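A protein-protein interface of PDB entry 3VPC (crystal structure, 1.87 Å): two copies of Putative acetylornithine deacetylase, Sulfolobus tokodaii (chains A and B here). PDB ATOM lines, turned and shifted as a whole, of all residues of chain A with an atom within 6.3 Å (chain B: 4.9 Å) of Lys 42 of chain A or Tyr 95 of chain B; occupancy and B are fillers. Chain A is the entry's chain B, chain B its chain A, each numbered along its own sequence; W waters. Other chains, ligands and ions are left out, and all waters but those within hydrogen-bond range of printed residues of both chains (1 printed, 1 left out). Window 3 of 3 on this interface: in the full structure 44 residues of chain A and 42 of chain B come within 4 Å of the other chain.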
ATOM      1  N   PRO A  39      -2.302  -8.565  15.595  1.00  0.00           N
ATOM      2  CA  PRO A  39      -1.362  -8.034  16.579  1.00  0.00           C
ATOM      3  C   PRO A  39      -1.280  -6.511  16.507  1.00  0.00           C
ATOM      4  O   PRO A  39      -1.492  -5.916  15.445  1.00  0.00           O
ATOM      5  CB  PRO A  39      -0.009  -8.647  16.165  1.00  0.00           C
ATOM      6  CG  PRO A  39      -0.154  -9.006  14.733  1.00  0.00           C
ATOM      7  CD  PRO A  39      -1.628  -9.286  14.495  1.00  0.00           C
ATOM      8  N   PHE A  40      -1.017  -5.887  17.649  1.00  0.00           N
ATOM      9  CA  PHE A  40      -0.568  -4.505  17.641  1.00  0.00           C
ATOM     10  C   PHE A  40       0.881  -4.580  17.218  1.00  0.00           C
ATOM     11  O   PHE A  40       1.751  -4.955  18.007  1.00  0.00           O
ATOM     12  CB  PHE A  40      -0.688  -3.867  19.022  1.00  0.00           C
ATOM     13  CG  PHE A  40      -2.070  -3.434  19.364  1.00  0.00           C
ATOM     14  CD1 PHE A  40      -2.820  -4.123  20.308  1.00  0.00           C
ATOM     15  CD2 PHE A  40      -2.638  -2.325  18.733  1.00  0.00           C
ATOM     16  CE1 PHE A  40      -4.116  -3.722  20.616  1.00  0.00           C
ATOM     17  CE2 PHE A  40      -3.915  -1.926  19.032  1.00  0.00           C
ATOM     18  CZ  PHE A  40      -4.664  -2.622  19.977  1.00  0.00           C
ATOM     19  N   ASN A  41       1.127  -4.260  15.958  1.00  0.00           N
ATOM     20  CA  ASN A  41       2.467  -4.362  15.384  1.00  0.00           C
ATOM     21  C   ASN A  41       2.594  -3.279  14.347  1.00  0.00           C
ATOM     22  O   ASN A  41       1.597  -2.648  13.989  1.00  0.00           O
ATOM     23  CB  ASN A  41       2.698  -5.754  14.762  1.00  0.00           C
ATOM     24  CG  ASN A  41       1.947  -5.957  13.447  1.00  0.00           C
ATOM     25  OD1 ASN A  41       1.906  -7.070  12.911  1.00  0.00           O
ATOM     26  ND2 ASN A  41       1.367  -4.885  12.908  1.00  0.00           N
ATOM     27  N   LYS A  42       3.789  -3.031  13.849  1.00  0.00           N
ATOM     28  CA  LYS A  42       3.865  -2.068  12.760  1.00  0.00           C
ATOM     29  C   LYS A  42       3.830  -2.761  11.389  1.00  0.00           C
ATOM     30  O   LYS A  42       3.733  -2.096  10.364  1.00  0.00           O
ATOM     31  CB  LYS A  42       5.019  -1.065  12.942  1.00  0.00           C
ATOM     32  CG  LYS A  42       4.728   0.032  14.015  1.00  0.00           C
ATOM     33  CD  LYS A  42       3.671   1.053  13.548  1.00  0.00           C
ATOM     34  CE  LYS A  42       3.384   2.165  14.582  1.00  0.00           C
ATOM     35  NZ  LYS A  42       2.178   2.982  14.223  1.00  0.00           N
ATOM     36  N   ALA A  43       3.840  -4.094  11.400  1.00  0.00           N
ATOM     37  CA  ALA A  43       3.705  -4.907  10.183  1.00  0.00           C
ATOM     38  C   ALA A  43       2.493  -4.545   9.317  1.00  0.00           C
ATOM     39  O   ALA A  43       2.648  -4.355   8.108  1.00  0.00           O
ATOM     40  CB  ALA A  43       3.678  -6.399  10.520  1.00  0.00           C
ATOM     41  N   LEU A  44       1.304  -4.447   9.932  1.00  0.00           N
ATOM     42  CA  LEU A  44       0.060  -4.097   9.206  1.00  0.00           C
ATOM     43  C   LEU A  44       0.124  -2.750   8.490  1.00  0.00           C
ATOM     44  O   LEU A  44      -0.706  -2.461   7.618  1.00  0.00           O
ATOM     45  CB  LEU A  44      -1.158  -4.128  10.136  1.00  0.00           C
ATOM     46  CG  LEU A  44      -1.651  -5.486  10.622  1.00  0.00           C
ATOM     47  CD1 LEU A  44      -2.604  -5.281  11.805  1.00  0.00           C
ATOM     48  CD2 LEU A  44      -2.314  -6.284   9.484  1.00  0.00           C
ATOM     49  N   GLY A  45       1.126  -1.944   8.841  1.00  0.00           N
ATOM     50  CA  GLY A  45       1.357  -0.651   8.214  1.00  0.00           C
ATOM     51  C   GLY A  45       1.687  -0.741   6.731  1.00  0.00           C
ATOM     52  O   GLY A  45       1.732   0.280   6.036  1.00  0.00           O
ATOM     53  N   ARG A  46       1.907  -1.968   6.255  1.00  0.00           N
ATOM     54  CA  ARG A  46       2.070  -2.235   4.819  1.00  0.00           C
ATOM     55  C   ARG A  46       0.813  -1.897   4.015  1.00  0.00           C
ATOM     56  O   ARG A  46       0.899  -1.638   2.822  1.00  0.00           O
ATOM     57  CB  ARG A  46       2.511  -3.683   4.557  1.00  0.00           C
ATOM     58  CG  ARG A  46       1.446  -4.744   4.772  1.00  0.00           C
ATOM     59  CD  ARG A  46       2.111  -6.104   4.841  1.00  0.00           C
ATOM     60  NE  ARG A  46       1.194  -7.211   5.091  1.00  0.00           N
ATOM     61  CZ  ARG A  46       0.818  -7.647   6.293  1.00  0.00           C
ATOM     62  NH1 ARG A  46      -0.014  -8.681   6.381  1.00  0.00           N
ATOM     63  NH2 ARG A  46       1.247  -7.051   7.402  1.00  0.00           N
ATOM     64  N   GLU A  68      -5.669   1.054  12.761  1.00  0.00           N
ATOM     65  CA  GLU A  68      -5.288   2.439  13.070  1.00  0.00           C
ATOM     66  C   GLU A  68      -4.000   2.550  13.889  1.00  0.00           C
ATOM     67  O   GLU A  68      -3.205   3.485  13.700  1.00  0.00           O
ATOM     68  CB  GLU A  68      -6.421   3.135  13.828  1.00  0.00           C
ATOM     69  CG  GLU A  68      -7.563   3.549  12.928  1.00  0.00           C
ATOM     70  CD  GLU A  68      -8.875   3.520  13.648  1.00  0.00           C
ATOM     71  OE1 GLU A  68      -9.899   3.324  12.972  1.00  0.00           O
ATOM     72  OE2 GLU A  68      -8.890   3.673  14.895  1.00  0.00           O
ATOM     73  N   ALA A  69      -3.780   1.577  14.773  1.00  0.00           N
ATOM     74  CA  ALA A  69      -2.603   1.568  15.653  1.00  0.00           C
ATOM     75  C   ALA A  69      -1.336   1.453  14.854  1.00  0.00           C
ATOM     76  O   ALA A  69      -0.301   2.002  15.254  1.00  0.00           O
ATOM     77  CB  ALA A  69      -2.691   0.409  16.668  1.00  0.00           C
ATOM     78  N   ALA A  70      -1.436   0.712  13.742  1.00  0.00           N
ATOM     79  CA  ALA A  70      -0.343   0.476  12.795  1.00  0.00           C
ATOM     80  C   ALA A  70      -0.252   1.576  11.735  1.00  0.00           C
ATOM     81  O   ALA A  70       0.627   1.546  10.866  1.00  0.00           O
ATOM     82  CB  ALA A  70      -0.554  -0.884  12.128  1.00  0.00           C
ATOM     83  N   GLY A  71      -1.173   2.533  11.799  1.00  0.00           N
ATOM     84  CA  GLY A  71      -1.145   3.731  10.958  1.00  0.00           C
ATOM     85  C   GLY A  71      -1.997   3.632   9.707  1.00  0.00           C
ATOM     86  O   GLY A  71      -1.946   4.539   8.851  1.00  0.00           O
ATOM     87  N   TYR B  91      -5.472   0.829  24.064  1.00  0.00           N
ATOM     88  CA  TYR B  91      -4.176   0.338  23.581  1.00  0.00           C
ATOM     89  C   TYR B  91      -3.877   0.870  22.173  1.00  0.00           C
ATOM     90  O   TYR B  91      -2.729   1.193  21.863  1.00  0.00           O
ATOM     91  CB  TYR B  91      -4.109  -1.197  23.583  1.00  0.00           C
ATOM     92  CG  TYR B  91      -4.086  -1.832  24.950  1.00  0.00           C
ATOM     93  CD1 TYR B  91      -4.759  -3.035  25.200  1.00  0.00           C
ATOM     94  CD2 TYR B  91      -3.415  -1.214  26.016  1.00  0.00           C
ATOM     95  CE1 TYR B  91      -4.748  -3.621  26.470  1.00  0.00           C
ATOM     96  CE2 TYR B  91      -3.378  -1.806  27.262  1.00  0.00           C
ATOM     97  CZ  TYR B  91      -4.052  -2.999  27.491  1.00  0.00           C
ATOM     98  OH  TYR B  91      -4.016  -3.552  28.755  1.00  0.00           O
ATOM     99  N   SER B  92      -4.914   0.953  21.347  1.00  0.00           N
ATOM    100  CA  SER B  92      -4.764   1.449  19.975  1.00  0.00           C
ATOM    101  C   SER B  92      -4.251   2.885  19.915  1.00  0.00           C
ATOM    102  O   SER B  92      -3.339   3.190  19.130  1.00  0.00           O
ATOM    103  CB  SER B  92      -6.084   1.317  19.217  1.00  0.00           C
ATOM    104  OG  SER B  92      -6.457  -0.042  19.132  1.00  0.00           O
ATOM    105  N   LYS B  93      -4.825   3.765  20.744  1.00  0.00           N
ATOM    106  CA  LYS B  93      -4.406   5.174  20.806  1.00  0.00           C
ATOM    107  C   LYS B  93      -2.982   5.305  21.328  1.00  0.00           C
ATOM    108  O   LYS B  93      -2.190   6.112  20.824  1.00  0.00           O
ATOM    109  CB  LYS B  93      -5.320   5.998  21.739  1.00  0.00           C
ATOM    110  CG  LYS B  93      -6.796   6.066  21.374  1.00  0.00           C
ATOM    111  CD  LYS B  93      -7.005   6.398  19.898  1.00  0.00           C
ATOM    112  CE  LYS B  93      -8.462   6.729  19.639  1.00  0.00           C
ATOM    113  NZ  LYS B  93      -8.768   6.820  18.188  1.00  0.00           N
ATOM    114  N   LEU B  94      -2.672   4.545  22.374  1.00  0.00           N
ATOM    115  CA  LEU B  94      -1.338   4.567  22.972  1.00  0.00           C
ATOM    116  C   LEU B  94      -0.282   3.980  22.013  1.00  0.00           C
ATOM    117  O   LEU B  94       0.767   4.581  21.793  1.00  0.00           O
ATOM    118  CB  LEU B  94      -1.328   3.799  24.297  1.00  0.00           C
ATOM    119  CG  LEU B  94      -2.283   4.325  25.383  1.00  0.00           C
ATOM    120  CD1 LEU B  94      -2.347   3.373  26.570  1.00  0.00           C
ATOM    121  CD2 LEU B  94      -1.874   5.718  25.856  1.00  0.00           C
ATOM    122  N   TYR B  95      -0.569   2.813  21.450  1.00  0.00           N
ATOM    123  CA  TYR B  95       0.362   2.172  20.529  1.00  0.00           C
ATOM    124  C   TYR B  95       0.718   3.047  19.326  1.00  0.00           C
ATOM    125  O   TYR B  95       1.902   3.125  18.936  1.00  0.00           O
ATOM    126  CB  TYR B  95      -0.154   0.800  20.056  1.00  0.00           C
ATOM    127  CG  TYR B  95       0.898   0.034  19.289  1.00  0.00           C
ATOM    128  CD1 TYR B  95       1.774  -0.824  19.952  1.00  0.00           C
ATOM    129  CD2 TYR B  95       1.047   0.197  17.907  1.00  0.00           C
ATOM    130  CE1 TYR B  95       2.759  -1.508  19.261  1.00  0.00           C
ATOM    131  CE2 TYR B  95       2.052  -0.485  17.203  1.00  0.00           C
ATOM    132  CZ  TYR B  95       2.894  -1.335  17.903  1.00  0.00           C
ATOM    133  OH  TYR B  95       3.875  -2.019  17.248  1.00  0.00           O
ATOM    134  N   ARG B  96      -0.290   3.697  18.744  1.00  0.00           N
ATOM    135  CA  ARG B  96      -0.081   4.595  17.606  1.00  0.00           C
ATOM    136  C   ARG B  96       0.914   5.706  17.955  1.00  0.00           C
ATOM    137  O   ARG B  96       1.712   6.141  17.110  1.00  0.00           O
ATOM    138  CB  ARG B  96      -1.426   5.181  17.156  1.00  0.00           C
ATOM    139  CG  ARG B  96      -1.374   6.290  16.112  1.00  0.00           C
ATOM    140  CD  ARG B  96      -0.800   5.828  14.779  1.00  0.00           C
ATOM    141  NE  ARG B  96      -1.207   6.715  13.687  1.00  0.00           N
ATOM    142  CZ  ARG B  96      -2.281   7.497  13.722  1.00  0.00           C
ATOM    143  NH1 ARG B  96      -3.079   7.489  14.783  1.00  0.00           N
ATOM    144  NH2 ARG B  96      -2.581   8.266  12.684  1.00  0.00           N
ATOM    145  N   GLU B  97       0.855   6.162  19.202  1.00  0.00           N
ATOM    146  CA  GLU B  97       1.722   7.229  19.675  1.00  0.00           C
ATOM    147  C   GLU B  97       3.060   6.760  20.225  1.00  0.00           C
ATOM    148  O   GLU B  97       3.887   7.585  20.607  1.00  0.00           O
ATOM    149  CB  GLU B  97       0.996   8.034  20.742  1.00  0.00           C
ATOM    150  CG  GLU B  97       0.002   9.008  20.174  1.00  0.00           C
ATOM    151  CD  GLU B  97       0.670  10.174  19.472  1.00  0.00           C
ATOM    152  OE1 GLU B  97       0.046  10.752  18.579  1.00  0.00           O
ATOM    153  OE2 GLU B  97       1.814  10.503  19.807  1.00  0.00           O
ATOM    154  N   GLY B  98       3.282   5.456  20.265  1.00  0.00           N
ATOM    155  CA  GLY B  98       4.539   4.909  20.769  1.00  0.00           C
ATOM    156  C   GLY B  98       4.648   4.889  22.281  1.00  0.00           C
ATOM    157  O   GLY B  98       5.748   4.786  22.819  1.00  0.00           O
ATOM    158  N   ILE B  99       3.507   4.993  22.967  1.00  0.00           N
ATOM    159  CA  ILE B  99       3.455   4.850  24.423  1.00  0.00           C
ATOM    160  C   ILE B  99       3.416   3.359  24.738  1.00  0.00           C
ATOM    161  O   ILE B  99       2.555   2.633  24.235  1.00  0.00           O
ATOM    162  CB  ILE B  99       2.239   5.594  25.019  1.00  0.00           C
ATOM    163  CG1 ILE B  99       2.314   7.085  24.646  1.00  0.00           C
ATOM    164  CG2 ILE B  99       2.142   5.406  26.531  1.00  0.00           C
ATOM    165  CD1 ILE B  99       1.126   7.868  25.144  1.00  0.00           C
ATOM    166  N   ILE B 101       2.829  -0.298  26.007  1.00  0.00           N
ATOM    167  CA  ILE B 101       1.699  -1.082  26.488  1.00  0.00           C
ATOM    168  C   ILE B 101       2.221  -2.529  26.594  1.00  0.00           C
ATOM    169  O   ILE B 101       3.293  -2.804  26.077  1.00  0.00           O
ATOM    170  CB  ILE B 101       0.491  -0.991  25.502  1.00  0.00           C
ATOM    171  CG1 ILE B 101       0.868  -1.550  24.118  1.00  0.00           C
ATOM    172  CG2 ILE B 101      -0.049   0.453  25.436  1.00  0.00           C
ATOM    173  CD1 ILE B 101      -0.337  -1.845  23.247  1.00  0.00           C
HETATM  174  O   HOH W   1      -7.487   4.308  17.224  1.00  0.00           O
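Of the printed residues of chain B, Lys 42 of chain A touches Tyr 95.
Tyr 95 of chain B touches just these residues of chain A: Phe 40, Asn 41, Lys 42 and Ala 69.
Printed residues of chain B within 4 Å of Glu 68 of chain A: Arg 96 (3.5 Å).
Of the printed residues of chain B, Ala 69 of chain A touches Ser 92, Tyr 95 and Arg 96.
Of the printed residues of chain A, Tyr 91 of chain B touches Phe 40 (3.9 Å).
Printed residues of chain A within 4 Å of Ser 92 of chain B: Phe 40 and Ala 69.
Printed residues of chain B within 4 Å of Phe 40 of chain A: Tyr 91, Ser 92 and Tyr 95.
Gly 71 of chain A touches none of the printed residues of chain B.
Of the 12 printed residues of chain A, 5 touch a printed residue of chain B.
Hydrophobic or aromatic side chains of chain A that line the printed part of chain B: Phe 40 and Ala 69.
Hydrophobic or aromatic side chains of chain B within 4 Å of the printed part of chain A: Tyr 91 and Tyr 95.
Along chain B the printed residues that touch a printed residue of chain A span positions 91 to 96.
Among the printed residues, 9 pairs touch across the chains.
Among the printed residues, no Asp or Glu carboxylate lies within 4 Å of a Lys or Arg side-chain nitrogen of the other chain.
The backbone carbonyl oxygen (O) of Ala 69 of chain A lies within hydrogen-bond range of the side-chain amino group (NZ) of Lys 42 of chain A (2.9 Å).
The side-chain amide nitrogen of Asn 41 of chain A sits close to the backbone NH of Leu 44 of chain A (3.0 Å).
The side-chain amide nitrogen (ND2) of Asn 41 of chain A sits close to the backbone NH (N) of Ala 43 of chain A.
Water W1 bridges the side-chain carboxylate of Glu 68 of chain A and the side-chain amino group of Lys 93 of chain B.
Phe 40 of chain A touches Tyr 91 of chain B (CE1 to CB, 3.9 Å).
Phe 40 of chain A touches Ser 92 of chain B (CE2 to OG, 3.2 Å).
O of Phe 40 of chain A touches OH of Tyr 95 of chain B, 3.7 Å away.
Asn 41 of chain A touches Tyr 95 of chain B (CA to OH, 3.3 Å).
OH of Tyr 95 of chain B touches N of Lys 42 of chain A, at 3.5 Å.
CD of Arg 96 of chain B touches O of Glu 68 of chain A (3.5 Å).
Ala 69 of chain A touches Ser 92 of chain B.
Tyr 95 of chain B touches Ala 69 of chain A.
O of Ala 69 of chain A touches CA of Arg 96 of chain B (3.5 Å).
No position is printed for both chains.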
